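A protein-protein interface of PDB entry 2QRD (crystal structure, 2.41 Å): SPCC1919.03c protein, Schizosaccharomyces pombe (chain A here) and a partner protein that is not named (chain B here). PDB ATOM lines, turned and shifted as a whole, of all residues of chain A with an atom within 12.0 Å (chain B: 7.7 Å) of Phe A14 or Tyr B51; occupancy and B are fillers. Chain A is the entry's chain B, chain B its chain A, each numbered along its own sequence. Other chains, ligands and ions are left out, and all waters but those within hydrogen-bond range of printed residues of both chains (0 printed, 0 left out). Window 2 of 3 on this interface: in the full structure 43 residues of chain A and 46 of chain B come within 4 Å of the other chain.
Hydrophobic or aromatic side chains of chain A that line the printed part of chain B: Ile A11, Pro A12, Phe A14, Leu A15, Leu A25 and Pro A26. Of the 17 printed residues of chain B, 9 touch a printed residue of chain A. Hydrophobic or aromatic side chains of chain B within 4 Å of the printed part of chain A: Pro B24, Leu B28, Tyr B31, Val B43, Pro B44, Tyr B51 and Met B55.
Leu B28 touches Ile A11. Tyr B31 touches Pro A12 (CD1 to CD, 3.98 Å). Val B43 touches Pro A12 (CG2 to CG, 3.7 Å). Pro A12 touches Pro B44 (CG to CD, 3.6 Å). Phe A14 touches Pro B44. O of Leu A15 touches CD2 of Leu B28 (3.4 Å). CD1 of Leu A25 touches CB of Pro B24, 3.9 Å away. Pro A26 touches Arg B52. CB of Pro A26 touches N of Ser B53, 3.7 Å away. Lys A27 touches Ser B53.
Phe A14 touches two residues of chain B. Of chain A, only Phe A14, Leu A25 and Pro A26 come within 4 Å of Tyr B51. No residue of chain B comes within 4 Å of Ala A13. Pro B44 touches just these residues of chain A: Pro A12 and Phe A14. No residue of chain A comes within 4 Å of Pro B46. No residue of chain A comes within 4 Å of Val B47. No residue of chain A comes within 4 Å of Gly B49. Arg B52 touches just one residue of chain A: Pro A26. Of chain A, only Pro A26 comes within 4 Å of Met B55. Printed residues of chain A within 4 Å of Pro B24: Leu A15 (3.99 Å) and Leu A25 (3.9 Å). Of the printed residues of chain B, Pro A26 touches Tyr B51 (3.5 Å), Arg B52 (3.5 Å), Ser B53 (3.7 Å) and Met B55 (3.9 Å). Printed residues of chain B within 4 Å of Thr A16: Leu B28 (3.9 Å). Of the printed residues of chain A, Leu B28 touches Ile A11, Leu A15 and Thr A16. Of the printed residues of chain A, Tyr B31 touches Pro A12 and Leu A15. Lys B45 touches none of the printed residues of chain A. Gln A21 touches none of the printed residues of chain B. The nearest residue of chain B that does not touch Phe A14 is Met B55 (4.4 Å). The nearest residue of chain A that does not touch Tyr B51 is Lys A24 (6.2 Å).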
ATOM      1  N   SER A   8      -1.301 -11.501  33.852  1.00  0.00           N
ATOM      2  CA  SER A   8      -2.629 -11.806  33.339  1.00  0.00           C
ATOM      3  C   SER A   8      -2.549 -12.712  32.104  1.00  0.00           C
ATOM      4  O   SER A   8      -1.546 -12.744  31.405  1.00  0.00           O
ATOM      5  CB  SER A   8      -3.359 -10.485  33.030  1.00  0.00           C
ATOM      6  OG  SER A   8      -4.742 -10.668  32.789  1.00  0.00           O
ATOM      7  N   GLU A  10      -5.533 -12.888  29.990  1.00  0.00           N
ATOM      8  CA  GLU A  10      -6.578 -12.353  29.116  1.00  0.00           C
ATOM      9  C   GLU A  10      -6.339 -10.903  28.635  1.00  0.00           C
ATOM     10  O   GLU A  10      -5.943 -10.015  29.412  1.00  0.00           O
ATOM     11  CB  GLU A  10      -7.949 -12.471  29.811  1.00  0.00           C
ATOM     12  CG  GLU A  10      -8.254 -13.858  30.415  1.00  0.00           C
ATOM     13  CD  GLU A  10      -8.340 -14.981  29.374  1.00  0.00           C
ATOM     14  OE1 GLU A  10      -7.316 -15.665  29.137  1.00  0.00           O
ATOM     15  OE2 GLU A  10      -9.435 -15.185  28.798  1.00  0.00           O
ATOM     16  N   ILE A  11      -6.616 -10.677  27.351  1.00  0.00           N
ATOM     17  CA  ILE A  11      -6.464  -9.360  26.718  1.00  0.00           C
ATOM     18  C   ILE A  11      -7.380  -8.300  27.385  1.00  0.00           C
ATOM     19  O   ILE A  11      -8.550  -8.575  27.668  1.00  0.00           O
ATOM     20  CB  ILE A  11      -6.728  -9.458  25.166  1.00  0.00           C
ATOM     21  CG1 ILE A  11      -5.787 -10.484  24.519  1.00  0.00           C
ATOM     22  CG2 ILE A  11      -6.563  -8.103  24.464  1.00  0.00           C
ATOM     23  CD1 ILE A  11      -6.458 -11.308  23.432  1.00  0.00           C
ATOM     24  N   PRO A  12      -6.843  -7.089  27.645  1.00  0.00           N
ATOM     25  CA  PRO A  12      -7.708  -6.060  28.236  1.00  0.00           C
ATOM     26  C   PRO A  12      -8.887  -5.757  27.323  1.00  0.00           C
ATOM     27  O   PRO A  12      -8.729  -5.696  26.104  1.00  0.00           O
ATOM     28  CB  PRO A  12      -6.790  -4.841  28.368  1.00  0.00           C
ATOM     29  CG  PRO A  12      -5.377  -5.403  28.309  1.00  0.00           C
ATOM     30  CD  PRO A  12      -5.462  -6.604  27.423  1.00  0.00           C
ATOM     31  N   ALA A  13     -10.055  -5.572  27.928  1.00  0.00           N
ATOM     32  CA  ALA A  13     -11.323  -5.501  27.211  1.00  0.00           C
ATOM     33  C   ALA A  13     -11.597  -4.141  26.562  1.00  0.00           C
ATOM     34  O   ALA A  13     -12.285  -4.077  25.547  1.00  0.00           O
ATOM     35  CB  ALA A  13     -12.472  -5.911  28.139  1.00  0.00           C
ATOM     36  N   PHE A  14     -11.050  -3.066  27.125  1.00  0.00           N
ATOM     37  CA  PHE A  14     -11.195  -1.747  26.527  1.00  0.00           C
ATOM     38  C   PHE A  14     -10.495  -1.657  25.161  1.00  0.00           C
ATOM     39  O   PHE A  14     -10.869  -0.836  24.339  1.00  0.00           O
ATOM     40  CB  PHE A  14     -10.724  -0.645  27.487  1.00  0.00           C
ATOM     41  CG  PHE A  14      -9.222  -0.523  27.605  1.00  0.00           C
ATOM     42  CD1 PHE A  14      -8.480  -1.448  28.350  1.00  0.00           C
ATOM     43  CD2 PHE A  14      -8.549   0.532  26.984  1.00  0.00           C
ATOM     44  CE1 PHE A  14      -7.082  -1.343  28.447  1.00  0.00           C
ATOM     45  CE2 PHE A  14      -7.157   0.648  27.070  1.00  0.00           C
ATOM     46  CZ  PHE A  14      -6.423  -0.293  27.803  1.00  0.00           C
ATOM     47  N   LEU A  15      -9.492  -2.514  24.926  1.00  0.00           N
ATOM     48  CA  LEU A  15      -8.781  -2.607  23.634  1.00  0.00           C
ATOM     49  C   LEU A  15      -9.532  -3.475  22.598  1.00  0.00           C
ATOM     50  O   LEU A  15      -9.280  -3.390  21.397  1.00  0.00           O
ATOM     51  CB  LEU A  15      -7.359  -3.149  23.831  1.00  0.00           C
ATOM     52  CG  LEU A  15      -6.324  -2.401  24.686  1.00  0.00           C
ATOM     53  CD1 LEU A  15      -5.123  -3.271  24.935  1.00  0.00           C
ATOM     54  CD2 LEU A  15      -5.878  -1.097  24.047  1.00  0.00           C
ATOM     55  N   THR A  16     -10.467  -4.289  23.080  1.00  0.00           N
ATOM     56  CA  THR A  16     -11.230  -5.220  22.246  1.00  0.00           C
ATOM     57  C   THR A  16     -12.567  -4.604  21.779  1.00  0.00           C
ATOM     58  O   THR A  16     -13.320  -5.225  21.018  1.00  0.00           O
ATOM     59  CB  THR A  16     -11.367  -6.593  22.995  1.00  0.00           C
ATOM     60  OG1 THR A  16     -10.104  -7.286  22.948  1.00  0.00           O
ATOM     61  CG2 THR A  16     -12.460  -7.489  22.420  1.00  0.00           C
ATOM     62  N   SER A  17     -12.833  -3.366  22.214  1.00  0.00           N
ATOM     63  CA  SER A  17     -14.055  -2.628  21.844  1.00  0.00           C
ATOM     64  C   SER A  17     -13.908  -1.864  20.515  1.00  0.00           C
ATOM     65  O   SER A  17     -12.837  -1.327  20.203  1.00  0.00           O
ATOM     66  CB  SER A  17     -14.458  -1.666  22.970  1.00  0.00           C
ATOM     67  OG  SER A  17     -15.857  -1.394  22.968  1.00  0.00           O
ATOM     68  N   ASN A  18     -15.005  -1.826  19.748  1.00  0.00           N
ATOM     69  CA  ASN A  18     -15.092  -1.130  18.451  1.00  0.00           C
ATOM     70  C   ASN A  18     -14.764   0.364  18.527  1.00  0.00           C
ATOM     71  O   ASN A  18     -15.331   1.103  19.336  1.00  0.00           O
ATOM     72  CB  ASN A  18     -16.468  -1.331  17.849  1.00  0.00           C
ATOM     73  N   GLN A  21     -11.184   2.590  20.359  1.00  0.00           N
ATOM     74  CA  GLN A  21     -11.074   2.973  18.953  1.00  0.00           C
ATOM     75  C   GLN A  21     -11.676   4.358  18.715  1.00  0.00           C
ATOM     76  O   GLN A  21     -11.122   5.172  17.970  1.00  0.00           O
ATOM     77  CB  GLN A  21     -11.751   1.935  18.062  1.00  0.00           C
ATOM     78  N   GLU A  22     -12.831   4.595  19.333  1.00  0.00           N
ATOM     79  CA  GLU A  22     -13.411   5.925  19.453  1.00  0.00           C
ATOM     80  C   GLU A  22     -13.215   6.408  20.896  1.00  0.00           C
ATOM     81  O   GLU A  22     -13.944   7.284  21.382  1.00  0.00           O
ATOM     82  CB  GLU A  22     -14.894   5.896  19.085  1.00  0.00           C
ATOM     83  N   LEU A  23     -12.226   5.810  21.568  1.00  0.00           N
ATOM     84  CA  LEU A  23     -11.893   6.113  22.958  1.00  0.00           C
ATOM     85  C   LEU A  23     -10.702   7.066  22.982  1.00  0.00           C
ATOM     86  O   LEU A  23      -9.829   6.977  22.117  1.00  0.00           O
ATOM     87  CB  LEU A  23     -11.575   4.829  23.716  1.00  0.00           C
ATOM     88  N   LYS A  24     -10.673   7.977  23.959  1.00  0.00           N
ATOM     89  CA  LYS A  24      -9.634   9.016  24.025  1.00  0.00           C
ATOM     90  C   LYS A  24      -8.444   8.563  24.851  1.00  0.00           C
ATOM     91  O   LYS A  24      -8.438   8.736  26.072  1.00  0.00           O
ATOM     92  N   LEU A  25      -7.431   8.002  24.181  1.00  0.00           N
ATOM     93  CA  LEU A  25      -6.315   7.314  24.859  1.00  0.00           C
ATOM     94  C   LEU A  25      -4.996   8.083  24.826  1.00  0.00           C
ATOM     95  O   LEU A  25      -4.803   8.923  23.948  1.00  0.00           O
ATOM     96  CB  LEU A  25      -6.121   5.906  24.281  1.00  0.00           C
ATOM     97  CG  LEU A  25      -7.220   4.937  24.729  1.00  0.00           C
ATOM     98  CD1 LEU A  25      -7.322   3.693  23.838  1.00  0.00           C
ATOM     99  CD2 LEU A  25      -7.110   4.581  26.238  1.00  0.00           C
ATOM    100  N   PRO A  26      -4.099   7.817  25.803  1.00  0.00           N
ATOM    101  CA  PRO A  26      -2.762   8.425  25.831  1.00  0.00           C
ATOM    102  C   PRO A  26      -1.813   7.882  24.758  1.00  0.00           C
ATOM    103  O   PRO A  26      -2.006   6.767  24.248  1.00  0.00           O
ATOM    104  CB  PRO A  26      -2.241   8.058  27.228  1.00  0.00           C
ATOM    105  CG  PRO A  26      -2.925   6.756  27.536  1.00  0.00           C
ATOM    106  CD  PRO A  26      -4.311   6.937  26.971  1.00  0.00           C
ATOM    107  N   LYS A  27      -0.800   8.694  24.443  1.00  0.00           N
ATOM    108  CA  LYS A  27       0.270   8.383  23.478  1.00  0.00           C
ATOM    109  C   LYS A  27       1.492   7.681  24.131  1.00  0.00           C
ATOM    110  O   LYS A  27       1.822   7.956  25.294  1.00  0.00           O
ATOM    111  CB  LYS A  27       0.716   9.681  22.792  1.00  0.00           C
ATOM    112  CG  LYS A  27      -0.260  10.182  21.733  1.00  0.00           C
ATOM    113  CD  LYS A  27       0.173  11.514  21.078  1.00  0.00           C
ATOM    114  CE  LYS A  27       1.385  11.354  20.152  1.00  0.00           C
ATOM    115  NZ  LYS A  27       1.596  12.511  19.204  1.00  0.00           N
ATOM    116  N   PRO A  28       2.179   6.787  23.379  1.00  0.00           N
ATOM    117  CA  PRO A  28       3.446   6.249  23.909  1.00  0.00           C
ATOM    118  C   PRO A  28       4.534   7.323  23.998  1.00  0.00           C
ATOM    119  O   PRO A  28       4.438   8.365  23.323  1.00  0.00           O
ATOM    120  CB  PRO A  28       3.836   5.157  22.898  1.00  0.00           C
ATOM    121  CG  PRO A  28       3.133   5.494  21.653  1.00  0.00           C
ATOM    122  CD  PRO A  28       1.862   6.231  22.045  1.00  0.00           C
ATOM    123  N   PRO A  29       5.559   7.084  24.839  1.00  0.00           N
ATOM    124  CA  PRO A  29       6.707   7.996  24.879  1.00  0.00           C
ATOM    125  C   PRO A  29       7.465   8.034  23.528  1.00  0.00           C
ATOM    126  O   PRO A  29       7.523   7.034  22.815  1.00  0.00           O
ATOM    127  CB  PRO A  29       7.589   7.393  25.991  1.00  0.00           C
ATOM    128  CG  PRO A  29       7.197   5.935  26.035  1.00  0.00           C
ATOM    129  CD  PRO A  29       5.718   5.960  25.785  1.00  0.00           C
ATOM    130  N   PRO B  24      -2.861   2.416  20.078  1.00  0.00           N
ATOM    131  CA  PRO B  24      -3.762   1.455  20.713  1.00  0.00           C
ATOM    132  C   PRO B  24      -4.067   0.208  19.849  1.00  0.00           C
ATOM    133  O   PRO B  24      -4.271  -0.874  20.406  1.00  0.00           O
ATOM    134  CB  PRO B  24      -5.026   2.276  20.968  1.00  0.00           C
ATOM    135  CG  PRO B  24      -4.584   3.690  20.897  1.00  0.00           C
ATOM    136  CD  PRO B  24      -3.559   3.689  19.838  1.00  0.00           C
ATOM    137  N   LEU B  27      -0.859  -1.769  20.345  1.00  0.00           N
ATOM    138  CA  LEU B  27      -0.869  -2.330  21.687  1.00  0.00           C
ATOM    139  C   LEU B  27      -1.752  -3.597  21.743  1.00  0.00           C
ATOM    140  O   LEU B  27      -1.281  -4.639  22.200  1.00  0.00           O
ATOM    141  CB  LEU B  27      -1.266  -1.272  22.731  1.00  0.00           C
ATOM    142  CG  LEU B  27      -1.139  -1.658  24.212  1.00  0.00           C
ATOM    143  CD1 LEU B  27       0.294  -2.100  24.576  1.00  0.00           C
ATOM    144  CD2 LEU B  27      -1.642  -0.535  25.144  1.00  0.00           C
ATOM    145  N   LEU B  28      -2.999  -3.502  21.258  1.00  0.00           N
ATOM    146  CA  LEU B  28      -3.876  -4.666  21.047  1.00  0.00           C
ATOM    147  C   LEU B  28      -3.205  -5.853  20.335  1.00  0.00           C
ATOM    148  O   LEU B  28      -3.327  -6.982  20.801  1.00  0.00           O
ATOM    149  CB  LEU B  28      -5.158  -4.272  20.271  1.00  0.00           C
ATOM    150  CG  LEU B  28      -6.213  -5.338  19.919  1.00  0.00           C
ATOM    151  CD1 LEU B  28      -6.861  -5.938  21.156  1.00  0.00           C
ATOM    152  CD2 LEU B  28      -7.302  -4.784  18.984  1.00  0.00           C
ATOM    153  N   TYR B  31      -0.633  -7.574  22.524  1.00  0.00           N
ATOM    154  CA  TYR B  31      -1.267  -8.398  23.562  1.00  0.00           C
ATOM    155  C   TYR B  31      -1.816  -9.679  22.980  1.00  0.00           C
ATOM    156  O   TYR B  31      -1.766 -10.735  23.603  1.00  0.00           O
ATOM    157  CB  TYR B  31      -2.397  -7.638  24.252  1.00  0.00           C
ATOM    158  CG  TYR B  31      -1.974  -6.835  25.464  1.00  0.00           C
ATOM    159  CD1 TYR B  31      -2.166  -5.460  25.506  1.00  0.00           C
ATOM    160  CD2 TYR B  31      -1.387  -7.448  26.575  1.00  0.00           C
ATOM    161  CE1 TYR B  31      -1.798  -4.709  26.642  1.00  0.00           C
ATOM    162  CE2 TYR B  31      -0.998  -6.697  27.707  1.00  0.00           C
ATOM    163  CZ  TYR B  31      -1.223  -5.335  27.733  1.00  0.00           C
ATOM    164  OH  TYR B  31      -0.845  -4.582  28.826  1.00  0.00           O
ATOM    165  N   VAL B  43      -1.099  -5.480  32.700  1.00  0.00           N
ATOM    166  CA  VAL B  43      -2.287  -4.954  32.062  1.00  0.00           C
ATOM    167  C   VAL B  43      -2.393  -3.457  32.433  1.00  0.00           C
ATOM    168  O   VAL B  43      -1.864  -3.049  33.472  1.00  0.00           O
ATOM    169  CB  VAL B  43      -3.508  -5.844  32.522  1.00  0.00           C
ATOM    170  CG1 VAL B  43      -4.668  -5.058  33.135  1.00  0.00           C
ATOM    171  CG2 VAL B  43      -3.901  -6.819  31.419  1.00  0.00           C
ATOM    172  N   PRO B  44      -3.033  -2.627  31.581  1.00  0.00           N
ATOM    173  CA  PRO B  44      -3.199  -1.217  31.941  1.00  0.00           C
ATOM    174  C   PRO B  44      -4.195  -1.028  33.076  1.00  0.00           C
ATOM    175  O   PRO B  44      -5.331  -1.542  33.019  1.00  0.00           O
ATOM    176  CB  PRO B  44      -3.764  -0.587  30.663  1.00  0.00           C
ATOM    177  CG  PRO B  44      -3.545  -1.599  29.583  1.00  0.00           C
ATOM    178  CD  PRO B  44      -3.618  -2.913  30.261  1.00  0.00           C
ATOM    179  N   LYS B  45      -3.758  -0.310  34.106  1.00  0.00           N
ATOM    180  CA  LYS B  45      -4.659   0.148  35.153  1.00  0.00           C
ATOM    181  C   LYS B  45      -4.933   1.646  34.927  1.00  0.00           C
ATOM    182  O   LYS B  45      -4.003   2.412  34.658  1.00  0.00           O
ATOM    183  CB  LYS B  45      -4.090  -0.164  36.557  1.00  0.00           C
ATOM    184  CG  LYS B  45      -4.954   0.307  37.775  1.00  0.00           C
ATOM    185  CD  LYS B  45      -6.342  -0.390  37.912  1.00  0.00           C
ATOM    186  CE  LYS B  45      -6.978  -0.094  39.280  1.00  0.00           C
ATOM    187  NZ  LYS B  45      -8.480  -0.249  39.368  1.00  0.00           N
ATOM    188  N   PRO B  46      -6.218   2.060  34.991  1.00  0.00           N
ATOM    189  CA  PRO B  46      -6.528   3.475  34.854  1.00  0.00           C
ATOM    190  C   PRO B  46      -6.451   4.228  36.190  1.00  0.00           C
ATOM    191  O   PRO B  46      -7.156   3.867  37.148  1.00  0.00           O
ATOM    192  CB  PRO B  46      -7.962   3.465  34.314  1.00  0.00           C
ATOM    193  CG  PRO B  46      -8.567   2.214  34.856  1.00  0.00           C
ATOM    194  CD  PRO B  46      -7.444   1.251  35.164  1.00  0.00           C
ATOM    195  N   VAL B  47      -5.599   5.257  36.244  1.00  0.00           N
ATOM    196  CA  VAL B  47      -5.439   6.094  37.448  1.00  0.00           C
ATOM    197  C   VAL B  47      -6.470   7.239  37.486  1.00  0.00           C
ATOM    198  O   VAL B  47      -6.452   8.146  36.641  1.00  0.00           O
ATOM    199  CB  VAL B  47      -3.946   6.574  37.664  1.00  0.00           C
ATOM    200  CG1 VAL B  47      -3.405   7.325  36.447  1.00  0.00           C
ATOM    201  CG2 VAL B  47      -3.796   7.399  38.961  1.00  0.00           C
ATOM    202  N   ASN B  48      -7.363   7.163  38.476  1.00  0.00           N
ATOM    203  CA  ASN B  48      -8.573   7.997  38.570  1.00  0.00           C
ATOM    204  C   ASN B  48      -9.547   7.837  37.393  1.00  0.00           C
ATOM    205  O   ASN B  48     -10.103   8.820  36.890  1.00  0.00           O
ATOM    206  CB  ASN B  48      -8.245   9.474  38.860  1.00  0.00           C
ATOM    207  CG  ASN B  48      -8.716   9.920  40.249  1.00  0.00           C
ATOM    208  OD1 ASN B  48      -9.548  10.820  40.370  1.00  0.00           O
ATOM    209  ND2 ASN B  48      -8.197   9.282  41.295  1.00  0.00           N
ATOM    210  N   GLY B  49      -9.756   6.585  36.981  1.00  0.00           N
ATOM    211  CA  GLY B  49     -10.660   6.254  35.872  1.00  0.00           C
ATOM    212  C   GLY B  49     -10.038   6.380  34.486  1.00  0.00           C
ATOM    213  O   GLY B  49     -10.544   5.792  33.515  1.00  0.00           O
ATOM    214  N   LYS B  50      -8.941   7.140  34.395  1.00  0.00           N
ATOM    215  CA  LYS B  50      -8.316   7.499  33.118  1.00  0.00           C
ATOM    216  C   LYS B  50      -7.034   6.700  32.890  1.00  0.00           C
ATOM    217  O   LYS B  50      -6.313   6.410  33.843  1.00  0.00           O
ATOM    218  CB  LYS B  50      -8.026   9.004  33.073  1.00  0.00           C
ATOM    219  N   TYR B  51      -6.750   6.363  31.631  1.00  0.00           N
ATOM    220  CA  TYR B  51      -5.538   5.603  31.269  1.00  0.00           C
ATOM    221  C   TYR B  51      -4.295   6.489  31.125  1.00  0.00           C
ATOM    222  O   TYR B  51      -4.381   7.631  30.653  1.00  0.00           O
ATOM    223  CB  TYR B  51      -5.760   4.757  29.999  1.00  0.00           C
ATOM    224  CG  TYR B  51      -6.657   3.569  30.236  1.00  0.00           C
ATOM    225  CD1 TYR B  51      -8.033   3.645  29.994  1.00  0.00           C
ATOM    226  CD2 TYR B  51      -6.142   2.381  30.735  1.00  0.00           C
ATOM    227  CE1 TYR B  51      -8.872   2.559  30.244  1.00  0.00           C
ATOM    228  CE2 TYR B  51      -6.964   1.291  30.980  1.00  0.00           C
ATOM    229  CZ  TYR B  51      -8.325   1.384  30.734  1.00  0.00           C
ATOM    230  OH  TYR B  51      -9.133   0.304  30.986  1.00  0.00           O
ATOM    231  N   ARG B  52      -3.149   5.944  31.542  1.00  0.00           N
ATOM    232  CA  ARG B  52      -1.863   6.641  31.478  1.00  0.00           C
ATOM    233  C   ARG B  52      -1.021   6.024  30.374  1.00  0.00           C
ATOM    234  O   ARG B  52      -1.245   4.877  30.007  1.00  0.00           O
ATOM    235  CB  ARG B  52      -1.138   6.531  32.812  1.00  0.00           C
ATOM    236  N   SER B  53      -0.045   6.771  29.861  1.00  0.00           N
ATOM    237  CA  SER B  53       0.824   6.264  28.805  1.00  0.00           C
ATOM    238  C   SER B  53       1.692   5.089  29.255  1.00  0.00           C
ATOM    239  O   SER B  53       2.355   4.473  28.435  1.00  0.00           O
ATOM    240  CB  SER B  53       1.686   7.379  28.224  1.00  0.00           C
ATOM    241  OG  SER B  53       2.490   7.963  29.225  1.00  0.00           O
ATOM    242  N   ASP B  54       1.673   4.774  30.555  1.00  0.00           N
ATOM    243  CA  ASP B  54       2.380   3.594  31.061  1.00  0.00           C
ATOM    244  C   ASP B  54       1.713   2.299  30.596  1.00  0.00           C
ATOM    245  O   ASP B  54       2.292   1.226  30.673  1.00  0.00           O
ATOM    246  CB  ASP B  54       2.591   3.637  32.583  1.00  0.00           C
ATOM    247  CG  ASP B  54       1.281   3.565  33.389  1.00  0.00           C
ATOM    248  OD1 ASP B  54       1.379   3.747  34.621  1.00  0.00           O
ATOM    249  OD2 ASP B  54       0.171   3.320  32.840  1.00  0.00           O
ATOM    250  N   MET B  55       0.509   2.428  30.056  1.00  0.00           N
ATOM    251  CA  MET B  55      -0.150   1.325  29.346  1.00  0.00           C
ATOM    252  C   MET B  55       0.713   0.744  28.214  1.00  0.00           C
ATOM    253  O   MET B  55       0.520  -0.405  27.829  1.00  0.00           O
ATOM    254  CB  MET B  55      -1.572   1.725  28.875  1.00  0.00           C
ATOM    255  CG  MET B  55      -1.674   2.536  27.585  1.00  0.00           C
ATOM    256  SD  MET B  55      -3.394   2.883  27.192  1.00  0.00           S
ATOM    257  CE  MET B  55      -3.418   2.953  25.407  1.00  0.00           C
